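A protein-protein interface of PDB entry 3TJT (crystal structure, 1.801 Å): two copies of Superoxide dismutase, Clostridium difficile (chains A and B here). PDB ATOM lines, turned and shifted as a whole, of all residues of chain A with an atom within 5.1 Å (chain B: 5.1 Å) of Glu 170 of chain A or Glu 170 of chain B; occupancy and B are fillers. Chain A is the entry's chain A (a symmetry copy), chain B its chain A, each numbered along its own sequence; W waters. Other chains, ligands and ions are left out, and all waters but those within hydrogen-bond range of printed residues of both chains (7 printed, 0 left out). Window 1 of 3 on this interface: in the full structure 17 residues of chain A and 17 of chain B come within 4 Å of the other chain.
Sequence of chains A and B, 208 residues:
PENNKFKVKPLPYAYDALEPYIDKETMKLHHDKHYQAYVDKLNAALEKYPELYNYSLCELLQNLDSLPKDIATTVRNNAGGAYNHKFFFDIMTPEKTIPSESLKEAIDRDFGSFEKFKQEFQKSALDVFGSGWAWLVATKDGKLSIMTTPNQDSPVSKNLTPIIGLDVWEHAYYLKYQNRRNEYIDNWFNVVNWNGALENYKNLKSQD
A ring nitrogen (NE2) of His 34 of chain B is in hydrogen-bond range of the side-chain hydroxyl of Tyr 174 of chain A (2.7 Å). The side-chain hydroxyl (OG) of Ser 131 of chain B sits at hydrogen-bond distance from the side-chain hydroxyl (OG) of Ser 131 of chain A (2.8 Å). The side-chain carboxylate (OE1) of Glu 170 of chain B lies within hydrogen-bond range of the backbone NH (N) of Glu 170 of chain A (3.4 Å). The side-chain carboxylate (OE2) of Glu 170 of chain B lies within hydrogen-bond range of a ring nitrogen (ND1) of His 171 of chain A (2.8 Å). OE2 of Glu 170 of chain A sits at hydrogen-bond distance from ND1 of His 171 of chain B, 2.8 Å away. A ring nitrogen (NE2) of His 34 of chain A is in hydrogen-bond range of the side-chain hydroxyl (OH) of Tyr 174 of chain B.
Among the printed residues, merely in contact across the chains: His 34 of chain A with Glu 170 of chain B, Trp 169 of chain A with Glu 170 of chain B, Glu 170 of chain A with His 34 of chain B, Glu 170 of chain A with Trp 169 of chain B, His 171 of chain A with Tyr 174 of chain B and Tyr 174 of chain A with His 171 of chain B.
Glu 170 of chain B touches just these residues of chain A: His 34 (3.8 Å), Trp 169 (3.8 Å), Glu 170 (3.4 Å) and His 171 (2.8 Å). Printed residues of chain B within 4 Å of His 171 of chain A: Glu 170 (2.8 Å) and Tyr 174 (3.5 Å). Of the printed residues of chain B, Tyr 174 of chain A touches His 34 (2.7 Å) and His 171 (3.5 Å). Of the printed residues of chain A, Trp 169 of chain B touches Glu 170. Of the printed residues of chain A, His 171 of chain B touches Glu 170 (2.8 Å) and Tyr 174 (3.5 Å). Printed residues of chain A within 4 Å of His 34 of chain B: Glu 170 (3.8 Å) and Tyr 174 (2.7 Å). Ala 172 of chain A touches none of the printed residues of chain B. The nearest residue of chain A that does not touch Glu 170 of chain B is Ser 131 of chain A (5.0 Å). The nearest printed residue of chain A that does not touch His 171 of chain B is His 171 of chain A (6.5 Å).
Of the 9 printed residues of chain B, 6 touch a printed residue of chain A. Printed residues of chain B that touch a printed residue of chain A: His 34, Ser 131, Trp 169, Glu 170, His 171 and Tyr 174.
His 34 of chain A touches Glu 170 of chain B, and with the chains exchanged Glu 170 of chain A touches His 34 of chain B. Ser 131 of chain B touches its own counterpart, Ser 131 of chain A. Trp 169 of chain A touches Glu 170 of chain B, and with the chains exchanged Glu 170 of chain A touches Trp 169 of chain B. Glu 170 of chain A touches His 171 of chain B, and with the chains exchanged His 171 of chain A touches Glu 170 of chain B. Positions printed for both chains: 34, 131, 168, 169, 170, 171, 172, 173 and 174.
Water W7 lies within hydrogen-bond range of the side-chain hydroxyl of Ser 131 of chain B (2.8 Å), the side-chain carboxylate of Glu 170 of chain A (2.8 Å) and the backbone NH of Glu 170 of chain B (2.8 Å). Water W6 lies within hydrogen-bond range of OG of Ser 131 of chain A (2.8 Å), OE1 of Glu 170 of chain B (2.8 Å) and N of Glu 170 of chain A (2.8 Å). Water W2 lies within hydrogen-bond range of OH of Tyr 174 of chain A (2.8 Å) and O of His 171 of chain B (2.9 Å). Water W5 lies within hydrogen-bond range of the side-chain hydroxyl (OH) of Tyr 174 of chain B (2.8 Å) and the backbone carbonyl oxygen (O) of His 171 of chain A (2.9 Å). Water W3 lies within hydrogen-bond range of a ring nitrogen (ND1) of His 34 of chain B (3.0 Å) and the side-chain carboxylate (OE2) of Glu 170 of chain A (3.4 Å). Water W1 lies within hydrogen-bond range of ND1 of His 34 of chain A (3.0 Å) and OE2 of Glu 170 of chain B (3.4 Å).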
ATOM      1  N   HIS A  34       2.294  25.753 -28.707  1.00  0.00           N
ATOM      2  CA  HIS A  34       2.271  27.148 -28.244  1.00  0.00           C
ATOM      3  C   HIS A  34       1.825  28.119 -29.341  1.00  0.00           C
ATOM      4  O   HIS A  34       0.887  28.886 -29.158  1.00  0.00           O
ATOM      5  CB  HIS A  34       3.630  27.579 -27.690  1.00  0.00           C
ATOM      6  CG  HIS A  34       4.044  26.848 -26.450  1.00  0.00           C
ATOM      7  ND1 HIS A  34       3.639  27.235 -25.188  1.00  0.00           N
ATOM      8  CD2 HIS A  34       4.834  25.761 -26.272  1.00  0.00           C
ATOM      9  CE1 HIS A  34       4.158  26.418 -24.290  1.00  0.00           C
ATOM     10  NE2 HIS A  34       4.889  25.514 -24.918  1.00  0.00           N
ATOM     11  N   SER A 131       8.882  36.261 -18.507  1.00  0.00           N
ATOM     12  CA  SER A 131       8.713  35.848 -19.906  1.00  0.00           C
ATOM     13  C   SER A 131       8.896  37.042 -20.827  1.00  0.00           C
ATOM     14  O   SER A 131       8.469  38.154 -20.502  1.00  0.00           O
ATOM     15  CB  SER A 131       7.308  35.277 -20.134  1.00  0.00           C
ATOM     16  OG  SER A 131       7.052  34.137 -19.300  1.00  0.00           O
ATOM     17  N   VAL A 168      12.675  34.325 -25.155  1.00  0.00           N
ATOM     18  CA  VAL A 168      13.272  33.836 -23.907  1.00  0.00           C
ATOM     19  C   VAL A 168      12.241  33.427 -22.855  1.00  0.00           C
ATOM     20  O   VAL A 168      12.559  33.360 -21.666  1.00  0.00           O
ATOM     21  CB  VAL A 168      14.341  34.799 -23.295  1.00  0.00           C
ATOM     22  CG1 VAL A 168      15.575  34.875 -24.192  1.00  0.00           C
ATOM     23  CG2 VAL A 168      13.764  36.192 -23.049  1.00  0.00           C
ATOM     24  N   TRP A 169      11.019  33.147 -23.293  1.00  0.00           N
ATOM     25  CA  TRP A 169      10.070  32.416 -22.454  1.00  0.00           C
ATOM     26  C   TRP A 169      10.752  31.100 -22.123  1.00  0.00           C
ATOM     27  O   TRP A 169      11.492  30.549 -22.950  1.00  0.00           O
ATOM     28  CB  TRP A 169       8.783  32.110 -23.209  1.00  0.00           C
ATOM     29  CG  TRP A 169       7.814  33.261 -23.339  1.00  0.00           C
ATOM     30  CD1 TRP A 169       8.055  34.486 -23.906  1.00  0.00           C
ATOM     31  CD2 TRP A 169       6.446  33.273 -22.923  1.00  0.00           C
ATOM     32  NE1 TRP A 169       6.916  35.260 -23.858  1.00  0.00           N
ATOM     33  CE2 TRP A 169       5.912  34.536 -23.270  1.00  0.00           C
ATOM     34  CE3 TRP A 169       5.615  32.338 -22.298  1.00  0.00           C
ATOM     35  CZ2 TRP A 169       4.585  34.886 -23.002  1.00  0.00           C
ATOM     36  CZ3 TRP A 169       4.286  32.683 -22.036  1.00  0.00           C
ATOM     37  CH2 TRP A 169       3.787  33.949 -22.388  1.00  0.00           C
ATOM     38  N   GLU A 170      10.497  30.570 -20.934  1.00  0.00           N
ATOM     39  CA  GLU A 170      11.144  29.319 -20.566  1.00  0.00           C
ATOM     40  C   GLU A 170      10.740  28.140 -21.461  1.00  0.00           C
ATOM     41  O   GLU A 170      11.538  27.217 -21.646  1.00  0.00           O
ATOM     42  CB  GLU A 170      10.946  29.033 -19.069  1.00  0.00           C
ATOM     43  CG  GLU A 170      11.808  29.961 -18.215  1.00  0.00           C
ATOM     44  CD  GLU A 170      11.480  29.915 -16.726  1.00  0.00           C
ATOM     45  OE1 GLU A 170      10.302  29.692 -16.365  1.00  0.00           O
ATOM     46  OE2 GLU A 170      12.418  30.109 -15.933  1.00  0.00           O
ATOM     47  N   HIS A 171       9.543  28.163 -22.038  1.00  0.00           N
ATOM     48  CA  HIS A 171       9.175  27.058 -22.932  1.00  0.00           C
ATOM     49  C   HIS A 171      10.129  26.943 -24.118  1.00  0.00           C
ATOM     50  O   HIS A 171      10.250  25.879 -24.727  1.00  0.00           O
ATOM     51  CB  HIS A 171       7.702  27.081 -23.385  1.00  0.00           C
ATOM     52  CG  HIS A 171       7.316  28.282 -24.201  1.00  0.00           C
ATOM     53  ND1 HIS A 171       6.326  29.157 -23.804  1.00  0.00           N
ATOM     54  CD2 HIS A 171       7.769  28.740 -25.392  1.00  0.00           C
ATOM     55  CE1 HIS A 171       6.187  30.105 -24.720  1.00  0.00           C
ATOM     56  NE2 HIS A 171       7.056  29.877 -25.687  1.00  0.00           N
ATOM     57  N   ALA A 172      10.826  28.026 -24.433  1.00  0.00           N
ATOM     58  CA  ALA A 172      11.672  28.032 -25.622  1.00  0.00           C
ATOM     59  C   ALA A 172      12.992  27.315 -25.410  1.00  0.00           C
ATOM     60  O   ALA A 172      13.680  26.982 -26.381  1.00  0.00           O
ATOM     61  CB  ALA A 172      11.932  29.461 -26.102  1.00  0.00           C
ATOM     62  N   TYR A 173      13.364  27.089 -24.152  1.00  0.00           N
ATOM     63  CA  TYR A 173      14.684  26.548 -23.870  1.00  0.00           C
ATOM     64  C   TYR A 173      14.786  25.555 -22.710  1.00  0.00           C
ATOM     65  O   TYR A 173      15.852  24.982 -22.504  1.00  0.00           O
ATOM     66  CB  TYR A 173      15.709  27.672 -23.656  1.00  0.00           C
ATOM     67  CG  TYR A 173      15.487  28.572 -22.442  1.00  0.00           C
ATOM     68  CD1 TYR A 173      15.959  28.212 -21.177  1.00  0.00           C
ATOM     69  CD2 TYR A 173      14.845  29.800 -22.576  1.00  0.00           C
ATOM     70  CE1 TYR A 173      15.783  29.068 -20.064  1.00  0.00           C
ATOM     71  CE2 TYR A 173      14.660  30.653 -21.472  1.00  0.00           C
ATOM     72  CZ  TYR A 173      15.127  30.282 -20.230  1.00  0.00           C
ATOM     73  OH  TYR A 173      14.945  31.132 -19.151  1.00  0.00           O
ATOM     74  N   TYR A 174      13.707  25.348 -21.961  1.00  0.00           N
ATOM     75  CA  TYR A 174      13.840  24.585 -20.717  1.00  0.00           C
ATOM     76  C   TYR A 174      14.170  23.095 -20.920  1.00  0.00           C
ATOM     77  O   TYR A 174      14.934  22.516 -20.145  1.00  0.00           O
ATOM     78  CB  TYR A 174      12.626  24.774 -19.785  1.00  0.00           C
ATOM     79  CG  TYR A 174      13.067  24.780 -18.337  1.00  0.00           C
ATOM     80  CD1 TYR A 174      13.700  25.889 -17.794  1.00  0.00           C
ATOM     81  CD2 TYR A 174      12.897  23.660 -17.533  1.00  0.00           C
ATOM     82  CE1 TYR A 174      14.140  25.898 -16.473  1.00  0.00           C
ATOM     83  CE2 TYR A 174      13.339  23.655 -16.200  1.00  0.00           C
ATOM     84  CZ  TYR A 174      13.960  24.772 -15.688  1.00  0.00           C
ATOM     85  OH  TYR A 174      14.401  24.779 -14.387  1.00  0.00           O
ATOM     86  N   HIS B  34      17.104  27.901  -9.232  1.00  0.00           N
ATOM     87  CA  HIS B  34      16.261  29.101  -9.322  1.00  0.00           C
ATOM     88  C   HIS B  34      16.140  29.831  -7.981  1.00  0.00           C
ATOM     89  O   HIS B  34      16.425  31.018  -7.883  1.00  0.00           O
ATOM     90  CB  HIS B  34      14.868  28.771  -9.861  1.00  0.00           C
ATOM     91  CG  HIS B  34      14.861  28.280 -11.277  1.00  0.00           C
ATOM     92  ND1 HIS B  34      14.852  29.136 -12.360  1.00  0.00           N
ATOM     93  CD2 HIS B  34      14.852  27.026 -11.791  1.00  0.00           C
ATOM     94  CE1 HIS B  34      14.840  28.430 -13.477  1.00  0.00           C
ATOM     95  NE2 HIS B  34      14.839  27.148 -13.162  1.00  0.00           N
ATOM     96  N   SER B 131       4.755  34.661 -16.954  1.00  0.00           N
ATOM     97  CA  SER B 131       5.252  34.090 -15.697  1.00  0.00           C
ATOM     98  C   SER B 131       4.479  34.664 -14.522  1.00  0.00           C
ATOM     99  O   SER B 131       4.138  35.851 -14.517  1.00  0.00           O
ATOM    100  CB  SER B 131       6.736  34.422 -15.504  1.00  0.00           C
ATOM    101  OG  SER B 131       7.543  33.909 -16.574  1.00  0.00           O
ATOM    102  N   VAL B 168       3.411  29.256 -11.360  1.00  0.00           N
ATOM    103  CA  VAL B 168       3.113  28.846 -12.736  1.00  0.00           C
ATOM    104  C   VAL B 168       4.094  29.406 -13.767  1.00  0.00           C
ATOM    105  O   VAL B 168       3.778  29.468 -14.957  1.00  0.00           O
ATOM    106  CB  VAL B 168       1.635  29.109 -13.173  1.00  0.00           C
ATOM    107  CG1 VAL B 168       0.675  28.212 -12.394  1.00  0.00           C
ATOM    108  CG2 VAL B 168       1.257  30.580 -13.008  1.00  0.00           C
ATOM    109  N   TRP B 169       5.278  29.801 -13.313  1.00  0.00           N
ATOM    110  CA  TRP B 169       6.400  30.011 -14.225  1.00  0.00           C
ATOM    111  C   TRP B 169       6.600  28.684 -14.936  1.00  0.00           C
ATOM    112  O   TRP B 169       6.400  27.616 -14.342  1.00  0.00           O
ATOM    113  CB  TRP B 169       7.678  30.345 -13.467  1.00  0.00           C
ATOM    114  CG  TRP B 169       7.789  31.765 -12.968  1.00  0.00           C
ATOM    115  CD1 TRP B 169       6.921  32.419 -12.132  1.00  0.00           C
ATOM    116  CD2 TRP B 169       8.846  32.686 -13.251  1.00  0.00           C
ATOM    117  NE1 TRP B 169       7.377  33.696 -11.886  1.00  0.00           N
ATOM    118  CE2 TRP B 169       8.561  33.882 -12.551  1.00  0.00           C
ATOM    119  CE3 TRP B 169      10.012  32.617 -14.020  1.00  0.00           C
ATOM    120  CZ2 TRP B 169       9.397  35.000 -12.609  1.00  0.00           C
ATOM    121  CZ3 TRP B 169      10.854  33.733 -14.072  1.00  0.00           C
ATOM    122  CH2 TRP B 169      10.538  34.908 -13.370  1.00  0.00           C
ATOM    123  N   GLU B 170       7.016  28.729 -16.194  1.00  0.00           N
ATOM    124  CA  GLU B 170       7.203  27.482 -16.921  1.00  0.00           C
ATOM    125  C   GLU B 170       8.298  26.589 -16.323  1.00  0.00           C
ATOM    126  O   GLU B 170       8.217  25.364 -16.446  1.00  0.00           O
ATOM    127  CB  GLU B 170       7.404  27.758 -18.420  1.00  0.00           C
ATOM    128  CG  GLU B 170       6.093  28.178 -19.080  1.00  0.00           C
ATOM    129  CD  GLU B 170       6.258  28.714 -20.499  1.00  0.00           C
ATOM    130  OE1 GLU B 170       7.305  29.328 -20.803  1.00  0.00           O
ATOM    131  OE2 GLU B 170       5.322  28.510 -21.293  1.00  0.00           O
ATOM    132  N   HIS B 171       9.295  27.166 -15.660  1.00  0.00           N
ATOM    133  CA  HIS B 171      10.318  26.309 -15.047  1.00  0.00           C
ATOM    134  C   HIS B 171       9.719  25.358 -14.014  1.00  0.00           C
ATOM    135  O   HIS B 171      10.301  24.315 -13.707  1.00  0.00           O
ATOM    136  CB  HIS B 171      11.526  27.080 -14.481  1.00  0.00           C
ATOM    137  CG  HIS B 171      11.197  28.022 -13.357  1.00  0.00           C
ATOM    138  ND1 HIS B 171      11.443  29.377 -13.434  1.00  0.00           N
ATOM    139  CD2 HIS B 171      10.663  27.804 -12.132  1.00  0.00           C
ATOM    140  CE1 HIS B 171      11.073  29.953 -12.300  1.00  0.00           C
ATOM    141  NE2 HIS B 171      10.591  29.021 -11.499  1.00  0.00           N
ATOM    142  N   ALA B 172       8.548  25.698 -13.495  1.00  0.00           N
ATOM    143  CA  ALA B 172       7.965  24.902 -12.420  1.00  0.00           C
ATOM    144  C   ALA B 172       7.309  23.628 -12.917  1.00  0.00           C
ATOM    145  O   ALA B 172       7.035  22.721 -12.124  1.00  0.00           O
ATOM    146  CB  ALA B 172       6.954  25.724 -11.616  1.00  0.00           C
ATOM    147  N   TYR B 173       7.037  23.554 -14.218  1.00  0.00           N
ATOM    148  CA  TYR B 173       6.272  22.433 -14.739  1.00  0.00           C
ATOM    149  C   TYR B 173       6.677  21.905 -16.117  1.00  0.00           C
ATOM    150  O   TYR B 173       6.141  20.889 -16.549  1.00  0.00           O
ATOM    151  CB  TYR B 173       4.768  22.744 -14.747  1.00  0.00           C
ATOM    152  CG  TYR B 173       4.314  23.873 -15.670  1.00  0.00           C
ATOM    153  CD1 TYR B 173       4.039  23.639 -17.020  1.00  0.00           C
ATOM    154  CD2 TYR B 173       4.117  25.160 -15.175  1.00  0.00           C
ATOM    155  CE1 TYR B 173       3.582  24.682 -17.861  1.00  0.00           C
ATOM    156  CE2 TYR B 173       3.669  26.203 -16.007  1.00  0.00           C
ATOM    157  CZ  TYR B 173       3.407  25.957 -17.338  1.00  0.00           C
ATOM    158  OH  TYR B 173       2.962  26.990 -18.146  1.00  0.00           O
ATOM    159  N   TYR B 174       7.603  22.572 -16.800  1.00  0.00           N
ATOM    160  CA  TYR B 174       7.841  22.224 -18.202  1.00  0.00           C
ATOM    161  C   TYR B 174       8.472  20.834 -18.412  1.00  0.00           C
ATOM    162  O   TYR B 174       8.133  20.136 -19.370  1.00  0.00           O
ATOM    163  CB  TYR B 174       8.626  23.320 -18.951  1.00  0.00           C
ATOM    164  CG  TYR B 174       8.146  23.431 -20.381  1.00  0.00           C
ATOM    165  CD1 TYR B 174       6.937  24.047 -20.678  1.00  0.00           C
ATOM    166  CD2 TYR B 174       8.874  22.876 -21.426  1.00  0.00           C
ATOM    167  CE1 TYR B 174       6.468  24.129 -21.986  1.00  0.00           C
ATOM    168  CE2 TYR B 174       8.410  22.949 -22.748  1.00  0.00           C
ATOM    169  CZ  TYR B 174       7.209  23.570 -23.012  1.00  0.00           C
ATOM    170  OH  TYR B 174       6.741  23.645 -24.301  1.00  0.00           O
HETATM  171  O   HOH W   1       2.853  29.496 -23.339  1.00  0.00           O
HETATM  172  O   HOH W   2      12.744  24.118 -12.192  1.00  0.00           O
HETATM  173  O   HOH W   3      13.994  31.802 -13.503  1.00  0.00           O
HETATM  174  O   HOH W   4       6.239  37.196 -17.482  1.00  0.00           O
HETATM  175  O   HOH W   5       8.276  24.671 -26.444  1.00  0.00           O
HETATM  176  O   HOH W   6       8.223  31.669 -19.667  1.00  0.00           O
HETATM  177  O   HOH W   7       8.089  31.234 -16.945  1.00  0.00           O
